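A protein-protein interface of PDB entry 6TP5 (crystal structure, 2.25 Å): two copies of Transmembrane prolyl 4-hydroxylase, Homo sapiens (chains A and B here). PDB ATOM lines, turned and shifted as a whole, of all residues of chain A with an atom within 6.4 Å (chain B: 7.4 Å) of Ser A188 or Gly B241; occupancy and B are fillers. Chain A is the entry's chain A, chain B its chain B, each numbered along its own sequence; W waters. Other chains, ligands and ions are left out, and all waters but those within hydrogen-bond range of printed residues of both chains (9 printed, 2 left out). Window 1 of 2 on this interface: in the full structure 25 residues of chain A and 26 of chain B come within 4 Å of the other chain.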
ATOM      1  N   TRP A 140      11.881  21.323 -13.166  1.00  0.00           N
ATOM      2  CA  TRP A 140      12.476  20.759 -11.964  1.00  0.00           C
ATOM      3  C   TRP A 140      11.732  21.309 -10.760  1.00  0.00           C
ATOM      4  O   TRP A 140      11.505  22.519 -10.663  1.00  0.00           O
ATOM      5  CB  TRP A 140      13.969  21.103 -11.879  1.00  0.00           C
ATOM      6  CG  TRP A 140      14.656  20.551 -10.652  1.00  0.00           C
ATOM      7  CD1 TRP A 140      15.103  21.262  -9.569  1.00  0.00           C
ATOM      8  CD2 TRP A 140      14.979  19.174 -10.388  1.00  0.00           C
ATOM      9  NE1 TRP A 140      15.687  20.415  -8.655  1.00  0.00           N
ATOM     10  CE2 TRP A 140      15.618  19.129  -9.127  1.00  0.00           C
ATOM     11  CE3 TRP A 140      14.793  17.975 -11.097  1.00  0.00           C
ATOM     12  CZ2 TRP A 140      16.071  17.933  -8.558  1.00  0.00           C
ATOM     13  CZ3 TRP A 140      15.243  16.786 -10.531  1.00  0.00           C
ATOM     14  CH2 TRP A 140      15.874  16.775  -9.270  1.00  0.00           C
ATOM     15  N   ALA A 185       8.873  30.128 -17.176  1.00  0.00           N
ATOM     16  CA  ALA A 185      10.083  30.025 -16.384  1.00  0.00           C
ATOM     17  C   ALA A 185      11.266  29.880 -17.324  1.00  0.00           C
ATOM     18  O   ALA A 185      11.108  29.663 -18.529  1.00  0.00           O
ATOM     19  CB  ALA A 185      10.004  28.853 -15.401  1.00  0.00           C
ATOM     20  N   GLU A 186      12.458  30.006 -16.759  1.00  0.00           N
ATOM     21  CA  GLU A 186      13.686  29.953 -17.532  1.00  0.00           C
ATOM     22  C   GLU A 186      14.304  28.561 -17.480  1.00  0.00           C
ATOM     23  O   GLU A 186      13.979  27.727 -16.628  1.00  0.00           O
ATOM     24  CB  GLU A 186      14.682  30.999 -17.029  1.00  0.00           C
ATOM     25  CG  GLU A 186      14.403  32.399 -17.550  1.00  0.00           C
ATOM     26  CD  GLU A 186      13.630  33.234 -16.557  1.00  0.00           C
ATOM     27  OE1 GLU A 186      13.770  32.978 -15.342  1.00  0.00           O
ATOM     28  OE2 GLU A 186      12.890  34.145 -16.985  1.00  0.00           O
ATOM     29  N   SER A 187      15.228  28.330 -18.409  1.00  0.00           N
ATOM     30  CA  SER A 187      15.911  27.046 -18.498  1.00  0.00           C
ATOM     31  C   SER A 187      16.641  26.676 -17.213  1.00  0.00           C
ATOM     32  O   SER A 187      16.890  25.491 -16.977  1.00  0.00           O
ATOM     33  CB  SER A 187      16.887  27.072 -19.671  1.00  0.00           C
ATOM     34  OG  SER A 187      17.885  28.052 -19.458  1.00  0.00           O
ATOM     35  N   SER A 188      16.999  27.647 -16.374  1.00  0.00           N
ATOM     36  CA  SER A 188      17.586  27.281 -15.091  1.00  0.00           C
ATOM     37  C   SER A 188      16.595  26.588 -14.159  1.00  0.00           C
ATOM     38  O   SER A 188      17.008  26.047 -13.130  1.00  0.00           O
ATOM     39  CB  SER A 188      18.166  28.521 -14.411  1.00  0.00           C
ATOM     40  OG  SER A 188      17.134  29.424 -14.083  1.00  0.00           O
ATOM     41  N   GLU A 189      15.307  26.587 -14.485  1.00  0.00           N
ATOM     42  CA  GLU A 189      14.309  25.867 -13.710  1.00  0.00           C
ATOM     43  C   GLU A 189      13.926  24.544 -14.355  1.00  0.00           C
ATOM     44  O   GLU A 189      12.965  23.904 -13.909  1.00  0.00           O
ATOM     45  CB  GLU A 189      13.072  26.746 -13.500  1.00  0.00           C
ATOM     46  CG  GLU A 189      13.442  28.124 -12.962  1.00  0.00           C
ATOM     47  CD  GLU A 189      12.246  28.986 -12.627  1.00  0.00           C
ATOM     48  OE1 GLU A 189      11.508  28.641 -11.684  1.00  0.00           O
ATOM     49  OE2 GLU A 189      12.056  30.022 -13.303  1.00  0.00           O
ATOM     50  N   LEU A 190      14.664  24.115 -15.382  1.00  0.00           N
ATOM     51  CA  LEU A 190      14.426  22.854 -16.069  1.00  0.00           C
ATOM     52  C   LEU A 190      15.252  21.732 -15.449  1.00  0.00           C
ATOM     53  O   LEU A 190      16.221  21.963 -14.718  1.00  0.00           O
ATOM     54  CB  LEU A 190      14.776  22.970 -17.549  1.00  0.00           C
ATOM     55  CG  LEU A 190      13.973  23.922 -18.418  1.00  0.00           C
ATOM     56  CD1 LEU A 190      14.614  23.987 -19.788  1.00  0.00           C
ATOM     57  CD2 LEU A 190      12.565  23.416 -18.514  1.00  0.00           C
ATOM     58  N   ASN A 193      19.558  21.933 -18.594  1.00  0.00           N
ATOM     59  CA  ASN A 193      19.748  23.347 -18.932  1.00  0.00           C
ATOM     60  C   ASN A 193      21.075  23.504 -19.674  1.00  0.00           C
ATOM     61  O   ASN A 193      22.103  23.849 -19.079  1.00  0.00           O
ATOM     62  CB  ASN A 193      19.704  24.182 -17.665  1.00  0.00           C
ATOM     63  CG  ASN A 193      19.976  25.648 -17.912  1.00  0.00           C
ATOM     64  OD1 ASN A 193      19.721  26.177 -19.002  1.00  0.00           O
ATOM     65  ND2 ASN A 193      20.489  26.322 -16.885  1.00  0.00           N
ATOM     66  N   GLY A 241      25.707  29.374 -15.727  1.00  0.00           N
ATOM     67  CA  GLY A 241      24.366  29.200 -15.203  1.00  0.00           C
ATOM     68  C   GLY A 241      23.709  27.890 -15.577  1.00  0.00           C
ATOM     69  O   GLY A 241      22.607  27.605 -15.089  1.00  0.00           O
ATOM     70  N   HIS A 243      23.262  23.639 -15.996  1.00  0.00           N
ATOM     71  CA  HIS A 243      23.215  22.564 -15.017  1.00  0.00           C
ATOM     72  C   HIS A 243      22.490  21.392 -15.664  1.00  0.00           C
ATOM     73  O   HIS A 243      21.825  21.535 -16.694  1.00  0.00           O
ATOM     74  CB  HIS A 243      22.467  22.994 -13.750  1.00  0.00           C
ATOM     75  CG  HIS A 243      20.980  22.970 -13.934  1.00  0.00           C
ATOM     76  ND1 HIS A 243      20.269  24.060 -14.391  1.00  0.00           N
ATOM     77  CD2 HIS A 243      20.085  21.962 -13.813  1.00  0.00           C
ATOM     78  CE1 HIS A 243      18.995  23.731 -14.514  1.00  0.00           C
ATOM     79  NE2 HIS A 243      18.858  22.462 -14.178  1.00  0.00           N
ATOM     80  N   HIS A 245      20.337  18.279 -13.637  1.00  0.00           N
ATOM     81  CA  HIS A 245      20.038  17.623 -12.371  1.00  0.00           C
ATOM     82  C   HIS A 245      20.254  16.118 -12.498  1.00  0.00           C
ATOM     83  O   HIS A 245      20.196  15.552 -13.596  1.00  0.00           O
ATOM     84  CB  HIS A 245      18.609  17.940 -11.930  1.00  0.00           C
ATOM     85  CG  HIS A 245      18.417  19.364 -11.503  1.00  0.00           C
ATOM     86  ND1 HIS A 245      19.113  19.927 -10.453  1.00  0.00           N
ATOM     87  CD2 HIS A 245      17.626  20.346 -11.999  1.00  0.00           C
ATOM     88  CE1 HIS A 245      18.748  21.190 -10.312  1.00  0.00           C
ATOM     89  NE2 HIS A 245      17.848  21.470 -11.239  1.00  0.00           N
ATOM     90  N   ARG A 320      22.164  22.170  -8.719  1.00  0.00           N
ATOM     91  CA  ARG A 320      22.366  23.603  -8.580  1.00  0.00           C
ATOM     92  C   ARG A 320      22.609  23.992  -7.131  1.00  0.00           C
ATOM     93  O   ARG A 320      23.280  24.994  -6.872  1.00  0.00           O
ATOM     94  CB  ARG A 320      21.157  24.373  -9.117  1.00  0.00           C
ATOM     95  CG  ARG A 320      20.942  24.276 -10.615  1.00  0.00           C
ATOM     96  CD  ARG A 320      19.801  25.186 -11.082  1.00  0.00           C
ATOM     97  NE  ARG A 320      20.107  26.601 -10.867  1.00  0.00           N
ATOM     98  CZ  ARG A 320      20.561  27.427 -11.809  1.00  0.00           C
ATOM     99  NH1 ARG A 320      20.766  26.991 -13.046  1.00  0.00           N
ATOM    100  NH2 ARG A 320      20.798  28.697 -11.516  1.00  0.00           N
ATOM    101  N   GLU B 186      22.302  30.518 -23.065  1.00  0.00           N
ATOM    102  CA  GLU B 186      21.162  30.506 -22.164  1.00  0.00           C
ATOM    103  C   GLU B 186      20.752  31.918 -21.762  1.00  0.00           C
ATOM    104  O   GLU B 186      21.499  32.887 -21.916  1.00  0.00           O
ATOM    105  CB  GLU B 186      21.476  29.696 -20.910  1.00  0.00           C
ATOM    106  CG  GLU B 186      22.309  28.464 -21.155  1.00  0.00           C
ATOM    107  CD  GLU B 186      21.579  27.409 -21.970  1.00  0.00           C
ATOM    108  OE1 GLU B 186      20.348  27.529 -22.163  1.00  0.00           O
ATOM    109  OE2 GLU B 186      22.244  26.447 -22.405  1.00  0.00           O
ATOM    110  N   SER B 187      19.542  32.020 -21.203  1.00  0.00           N
ATOM    111  CA  SER B 187      19.062  33.316 -20.727  1.00  0.00           C
ATOM    112  C   SER B 187      19.914  33.843 -19.574  1.00  0.00           C
ATOM    113  O   SER B 187      20.016  35.062 -19.387  1.00  0.00           O
ATOM    114  CB  SER B 187      17.593  33.220 -20.310  1.00  0.00           C
ATOM    115  OG  SER B 187      17.466  32.636 -19.025  1.00  0.00           O
ATOM    116  N   SER B 188      20.544  32.954 -18.803  1.00  0.00           N
ATOM    117  CA  SER B 188      21.473  33.408 -17.775  1.00  0.00           C
ATOM    118  C   SER B 188      22.736  34.059 -18.345  1.00  0.00           C
ATOM    119  O   SER B 188      23.550  34.558 -17.560  1.00  0.00           O
ATOM    120  CB  SER B 188      21.857  32.244 -16.863  1.00  0.00           C
ATOM    121  OG  SER B 188      22.475  31.210 -17.604  1.00  0.00           O
ATOM    122  N   ASN B 193      17.487  38.669 -17.422  1.00  0.00           N
ATOM    123  CA  ASN B 193      17.101  37.259 -17.347  1.00  0.00           C
ATOM    124  C   ASN B 193      15.873  37.143 -16.436  1.00  0.00           C
ATOM    125  O   ASN B 193      15.990  36.820 -15.251  1.00  0.00           O
ATOM    126  CB  ASN B 193      18.283  36.439 -16.838  1.00  0.00           C
ATOM    127  CG  ASN B 193      17.968  34.963 -16.699  1.00  0.00           C
ATOM    128  OD1 ASN B 193      17.071  34.437 -17.359  1.00  0.00           O
ATOM    129  ND2 ASN B 193      18.716  34.284 -15.837  1.00  0.00           N
ATOM    130  N   TYR B 238      11.435  36.836 -11.352  1.00  0.00           N
ATOM    131  CA  TYR B 238      12.765  36.242 -11.448  1.00  0.00           C
ATOM    132  C   TYR B 238      12.662  34.805 -10.969  1.00  0.00           C
ATOM    133  O   TYR B 238      12.440  34.564  -9.776  1.00  0.00           O
ATOM    134  CB  TYR B 238      13.780  36.986 -10.586  1.00  0.00           C
ATOM    135  CG  TYR B 238      14.158  38.367 -11.048  1.00  0.00           C
ATOM    136  CD1 TYR B 238      15.140  38.553 -12.015  1.00  0.00           C
ATOM    137  CD2 TYR B 238      13.557  39.489 -10.491  1.00  0.00           C
ATOM    138  CE1 TYR B 238      15.498  39.825 -12.430  1.00  0.00           C
ATOM    139  CE2 TYR B 238      13.910  40.764 -10.899  1.00  0.00           C
ATOM    140  CZ  TYR B 238      14.883  40.922 -11.864  1.00  0.00           C
ATOM    141  OH  TYR B 238      15.241  42.179 -12.268  1.00  0.00           O
ATOM    142  N   GLY B 239      12.823  33.852 -11.884  1.00  0.00           N
ATOM    143  CA  GLY B 239      12.941  32.467 -11.479  1.00  0.00           C
ATOM    144  C   GLY B 239      14.239  32.232 -10.724  1.00  0.00           C
ATOM    145  O   GLY B 239      15.107  33.103 -10.621  1.00  0.00           O
ATOM    146  N   GLU B 240      14.363  31.030 -10.162  1.00  0.00           N
ATOM    147  CA  GLU B 240      15.638  30.624  -9.585  1.00  0.00           C
ATOM    148  C   GLU B 240      16.696  30.631 -10.681  1.00  0.00           C
ATOM    149  O   GLU B 240      16.503  30.048 -11.754  1.00  0.00           O
ATOM    150  CB  GLU B 240      15.533  29.238  -8.937  1.00  0.00           C
ATOM    151  CG  GLU B 240      16.823  28.775  -8.237  1.00  0.00           C
ATOM    152  CD  GLU B 240      16.613  27.569  -7.316  1.00  0.00           C
ATOM    153  OE1 GLU B 240      15.506  27.430  -6.753  1.00  0.00           O
ATOM    154  OE2 GLU B 240      17.561  26.765  -7.139  1.00  0.00           O
ATOM    155  N   GLY B 241      17.800  31.322 -10.425  1.00  0.00           N
ATOM    156  CA  GLY B 241      18.794  31.549 -11.448  1.00  0.00           C
ATOM    157  C   GLY B 241      18.585  32.803 -12.269  1.00  0.00           C
ATOM    158  O   GLY B 241      19.345  33.031 -13.218  1.00  0.00           O
ATOM    159  N   GLY B 242      17.578  33.623 -11.937  1.00  0.00           N
ATOM    160  CA  GLY B 242      17.368  34.864 -12.649  1.00  0.00           C
ATOM    161  C   GLY B 242      18.256  35.988 -12.144  1.00  0.00           C
ATOM    162  O   GLY B 242      18.863  35.921 -11.072  1.00  0.00           O
ATOM    163  N   HIS B 243      18.317  37.055 -12.933  1.00  0.00           N
ATOM    164  CA  HIS B 243      19.232  38.158 -12.661  1.00  0.00           C
ATOM    165  C   HIS B 243      18.936  39.285 -13.643  1.00  0.00           C
ATOM    166  O   HIS B 243      18.310  39.083 -14.690  1.00  0.00           O
ATOM    167  CB  HIS B 243      20.694  37.730 -12.810  1.00  0.00           C
ATOM    168  CG  HIS B 243      21.156  37.710 -14.232  1.00  0.00           C
ATOM    169  ND1 HIS B 243      21.030  36.599 -15.040  1.00  0.00           N
ATOM    170  CD2 HIS B 243      21.701  38.680 -15.008  1.00  0.00           C
ATOM    171  CE1 HIS B 243      21.493  36.880 -16.248  1.00  0.00           C
ATOM    172  NE2 HIS B 243      21.896  38.140 -16.257  1.00  0.00           N
ATOM    173  N   GLY B 290      16.462  32.867  -1.295  1.00  0.00           N
ATOM    174  CA  GLY B 290      17.896  33.043  -1.464  1.00  0.00           C
ATOM    175  C   GLY B 290      18.305  34.068  -2.507  1.00  0.00           C
ATOM    176  O   GLY B 290      17.862  34.001  -3.658  1.00  0.00           O
ATOM    177  N   ARG B 320      25.400  38.611 -11.167  1.00  0.00           N
ATOM    178  CA  ARG B 320      25.471  37.186 -10.882  1.00  0.00           C
ATOM    179  C   ARG B 320      26.697  36.843 -10.057  1.00  0.00           C
ATOM    180  O   ARG B 320      26.653  35.909  -9.250  1.00  0.00           O
ATOM    181  CB  ARG B 320      25.503  36.373 -12.177  1.00  0.00           C
ATOM    182  CG  ARG B 320      24.235  36.436 -13.012  1.00  0.00           C
ATOM    183  CD  ARG B 320      24.354  35.524 -14.234  1.00  0.00           C
ATOM    184  NE  ARG B 320      24.426  34.112 -13.848  1.00  0.00           N
ATOM    185  CZ  ARG B 320      23.367  33.307 -13.744  1.00  0.00           C
ATOM    186  NH1 ARG B 320      22.146  33.770 -13.996  1.00  0.00           N
ATOM    187  NH2 ARG B 320      23.529  32.039 -13.393  1.00  0.00           N
ATOM    188  N   CYS B 363      20.212  41.106  -8.351  1.00  0.00           N
ATOM    189  CA  CYS B 363      21.178  40.069  -8.036  1.00  0.00           C
ATOM    190  C   CYS B 363      20.612  38.684  -8.317  1.00  0.00           C
ATOM    191  O   CYS B 363      19.399  38.461  -8.270  1.00  0.00           O
ATOM    192  CB  CYS B 363      21.584  40.164  -6.571  1.00  0.00           C
ATOM    193  SG  CYS B 363      22.421  41.724  -6.124  1.00  0.00           S
ATOM    194  N   LEU B 364      21.520  37.747  -8.594  1.00  0.00           N
ATOM    195  CA  LEU B 364      21.158  36.358  -8.840  1.00  0.00           C
ATOM    196  C   LEU B 364      20.274  35.813  -7.724  1.00  0.00           C
ATOM    197  O   LEU B 364      20.581  35.965  -6.537  1.00  0.00           O
ATOM    198  CB  LEU B 364      22.425  35.509  -8.964  1.00  0.00           C
ATOM    199  CG  LEU B 364      22.273  33.985  -9.044  1.00  0.00           C
ATOM    200  CD1 LEU B 364      21.802  33.586 -10.418  1.00  0.00           C
ATOM    201  CD2 LEU B 364      23.581  33.293  -8.719  1.00  0.00           C
ATOM    202  N   VAL B 365      19.175  35.176  -8.121  1.00  0.00           N
ATOM    203  CA  VAL B 365      18.278  34.490  -7.198  1.00  0.00           C
ATOM    204  C   VAL B 365      18.784  33.060  -7.031  1.00  0.00           C
ATOM    205  O   VAL B 365      18.817  32.290  -7.996  1.00  0.00           O
ATOM    206  CB  VAL B 365      16.829  34.520  -7.716  1.00  0.00           C
ATOM    207  CG1 VAL B 365      15.884  33.764  -6.780  1.00  0.00           C
ATOM    208  CG2 VAL B 365      16.365  35.967  -7.911  1.00  0.00           C
ATOM    209  N   THR B 366      19.178  32.701  -5.809  1.00  0.00           N
ATOM    210  CA  THR B 366      19.755  31.381  -5.566  1.00  0.00           C
ATOM    211  C   THR B 366      18.742  30.338  -5.100  1.00  0.00           C
ATOM    212  O   THR B 366      18.950  29.144  -5.341  1.00  0.00           O
ATOM    213  CB  THR B 366      20.869  31.474  -4.528  1.00  0.00           C
ATOM    214  OG1 THR B 366      20.344  32.039  -3.323  1.00  0.00           O
ATOM    215  CG2 THR B 366      22.015  32.331  -5.045  1.00  0.00           C
ATOM    216  N   ARG B 367      17.669  30.740  -4.417  1.00  0.00           N
ATOM    217  CA  ARG B 367      16.629  29.803  -4.000  1.00  0.00           C
ATOM    218  C   ARG B 367      15.269  30.428  -4.249  1.00  0.00           C
ATOM    219  O   ARG B 367      15.014  31.552  -3.810  1.00  0.00           O
ATOM    220  CB  ARG B 367      16.728  29.429  -2.507  1.00  0.00           C
ATOM    221  CG  ARG B 367      18.054  28.864  -2.053  1.00  0.00           C
ATOM    222  CD  ARG B 367      18.224  27.427  -2.485  1.00  0.00           C
ATOM    223  NE  ARG B 367      19.629  27.018  -2.515  1.00  0.00           N
ATOM    224  CZ  ARG B 367      20.262  26.411  -1.514  1.00  0.00           C
ATOM    225  NH1 ARG B 367      19.621  26.131  -0.382  1.00  0.00           N
ATOM    226  NH2 ARG B 367      21.542  26.076  -1.648  1.00  0.00           N
ATOM    227  N   GLY B 368      14.394  29.693  -4.918  1.00  0.00           N
ATOM    228  CA  GLY B 368      13.019  30.120  -5.022  1.00  0.00           C
ATOM    229  C   GLY B 368      12.816  31.137  -6.128  1.00  0.00           C
ATOM    230  O   GLY B 368      13.607  31.256  -7.069  1.00  0.00           O
HETATM  231  O   HOH W   1      21.054  30.412 -14.098  1.00  0.00           O
HETATM  232  O   HOH W   2      18.200  29.541 -22.037  1.00  0.00           O
HETATM  233  O   HOH W   3      20.620  30.080  -8.833  1.00  0.00           O
HETATM  234  O   HOH W   4      14.382  35.174 -19.182  1.00  0.00           O
HETATM  235  O   HOH W   5      18.659  31.234 -15.837  1.00  0.00           O
HETATM  236  O   HOH W   6      20.609  29.269 -16.990  1.00  0.00           O
HETATM  237  O   HOH W   7      26.150  30.683 -12.626  1.00  0.00           O
HETATM  238  O   HOH W   8      23.714  25.882 -20.275  1.00  0.00           O
HETATM  239  O   HOH W   9      19.963  27.301  -7.918  1.00  0.00           O
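Ser A188 touches just these residues of chain B: Glu B240 and Gly B241.
Gly B241 touches two residues of chain A.
Of the printed residues of chain B, Ser A187 touches Glu B186 (3.7 Å).
Of the printed residues of chain A, Glu B240 touches Ser A188 (2.5 Å) and Glu A189 (3.8 Å).
Of the printed residues of chain A, Ser B187 touches Glu A186.
Leu A190 touches none of the printed residues of chain B.
The nearest residue of chain A that does not touch Gly B241 is Glu A186 (5.7 Å).
Water W9 lies within hydrogen-bond range of OE2 of Glu B240 (2.6 Å), NE of Arg A320 (3.0 Å) and O of Thr B366 (3.3 Å).
Water W6 lies within hydrogen-bond range of the side-chain hydroxyl (OG) of Ser B188, the side-chain amide nitrogen (ND2) of Asn A193 and the backbone carbonyl oxygen (O) of Gly A241.
Water W4 bridges the side-chain carboxylate (OE2) of Glu A186 and the side-chain amide oxygen (OD1) of Asn B193.
Water W2 lies within hydrogen-bond range of N of Ser B187 (2.9 Å), OE1 of Glu B186 (2.9 Å) and OG of Ser A187 (3.0 Å).
Water W1 lies within hydrogen-bond range of NH2 of Arg B320 (3.0 Å), NH2 of Arg A320 (3.1 Å), O of Gly B241 (3.2 Å) and O of Gly A241 (3.4 Å).
Water W7 lies within hydrogen-bond range of NH2 of Arg B320 (3.0 Å) and N of Gly A241 (3.4 Å).
Among the printed residues, pairs that only touch across the chains: Glu A189 with Gly B239 (3.2 Å), Glu A186 with Asn B193 (3.4 Å), Glu A186 with Ser B187 (3.4 Å), Gly A241 with Arg B320 (3.5 Å), Arg A320 with Gly B241 (3.5 Å), Gly A241 with Ser B188 (3.7 Å), Glu A186 with Gly B239 (3.7 Å), Ser A187 with Glu B186 (3.7 Å), Ser A188 with Gly B241 (3.8 Å) and Glu A189 with Glu B240 (3.8 Å).
Printed residues of chain A that touch a printed residue of chain B: Glu A186, Ser A187, Ser A188, Glu A189, Asn A193, Gly A241 and Arg A320.
Glu A186 touches Ser B187, and with the chains exchanged Ser A187 touches Glu B186.
Glu A186 touches Asn B193, and with the chains exchanged Asn A193 touches Glu B186.
Ser A188 touches Gly B241, and with the chains exchanged Gly A241 touches Ser B188.
Gly A241 touches Arg B320, and with the chains exchanged Arg A320 touches Gly B241.
Positions printed for both chains: 186, 187, 188, 193, 241, 243 and 320.
OG of Ser A188 lies within hydrogen-bond range of O of Glu B240, at 2.5 Å.
The side-chain amide oxygen (OD1) of Asn A193 sits close to the side-chain carboxylate (OE1) of Glu B186.
N of Gly B368 is in hydrogen-bond range of OE1 of Glu B240 (3.1 Å).
A ring nitrogen (ND1) of His A243 lies within hydrogen-bond range of the guanidinium group of Arg A320 (3.3 Å).
The backbone carbonyl oxygen of Gly B241 is in hydrogen-bond range of the side-chain amide nitrogen of Asn B193 (3.0 Å).
The backbone carbonyl oxygen of Gly A241 is in hydrogen-bond range of the side-chain amide nitrogen of Asn A193.
The side-chain hydroxyl (OG) of Ser A187 is in hydrogen-bond range of the side-chain amide oxygen (OD1) of Asn A193, 2.7 Å away.
O of His A243 is in hydrogen-bond range of N of Asn A193 (3.0 Å).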
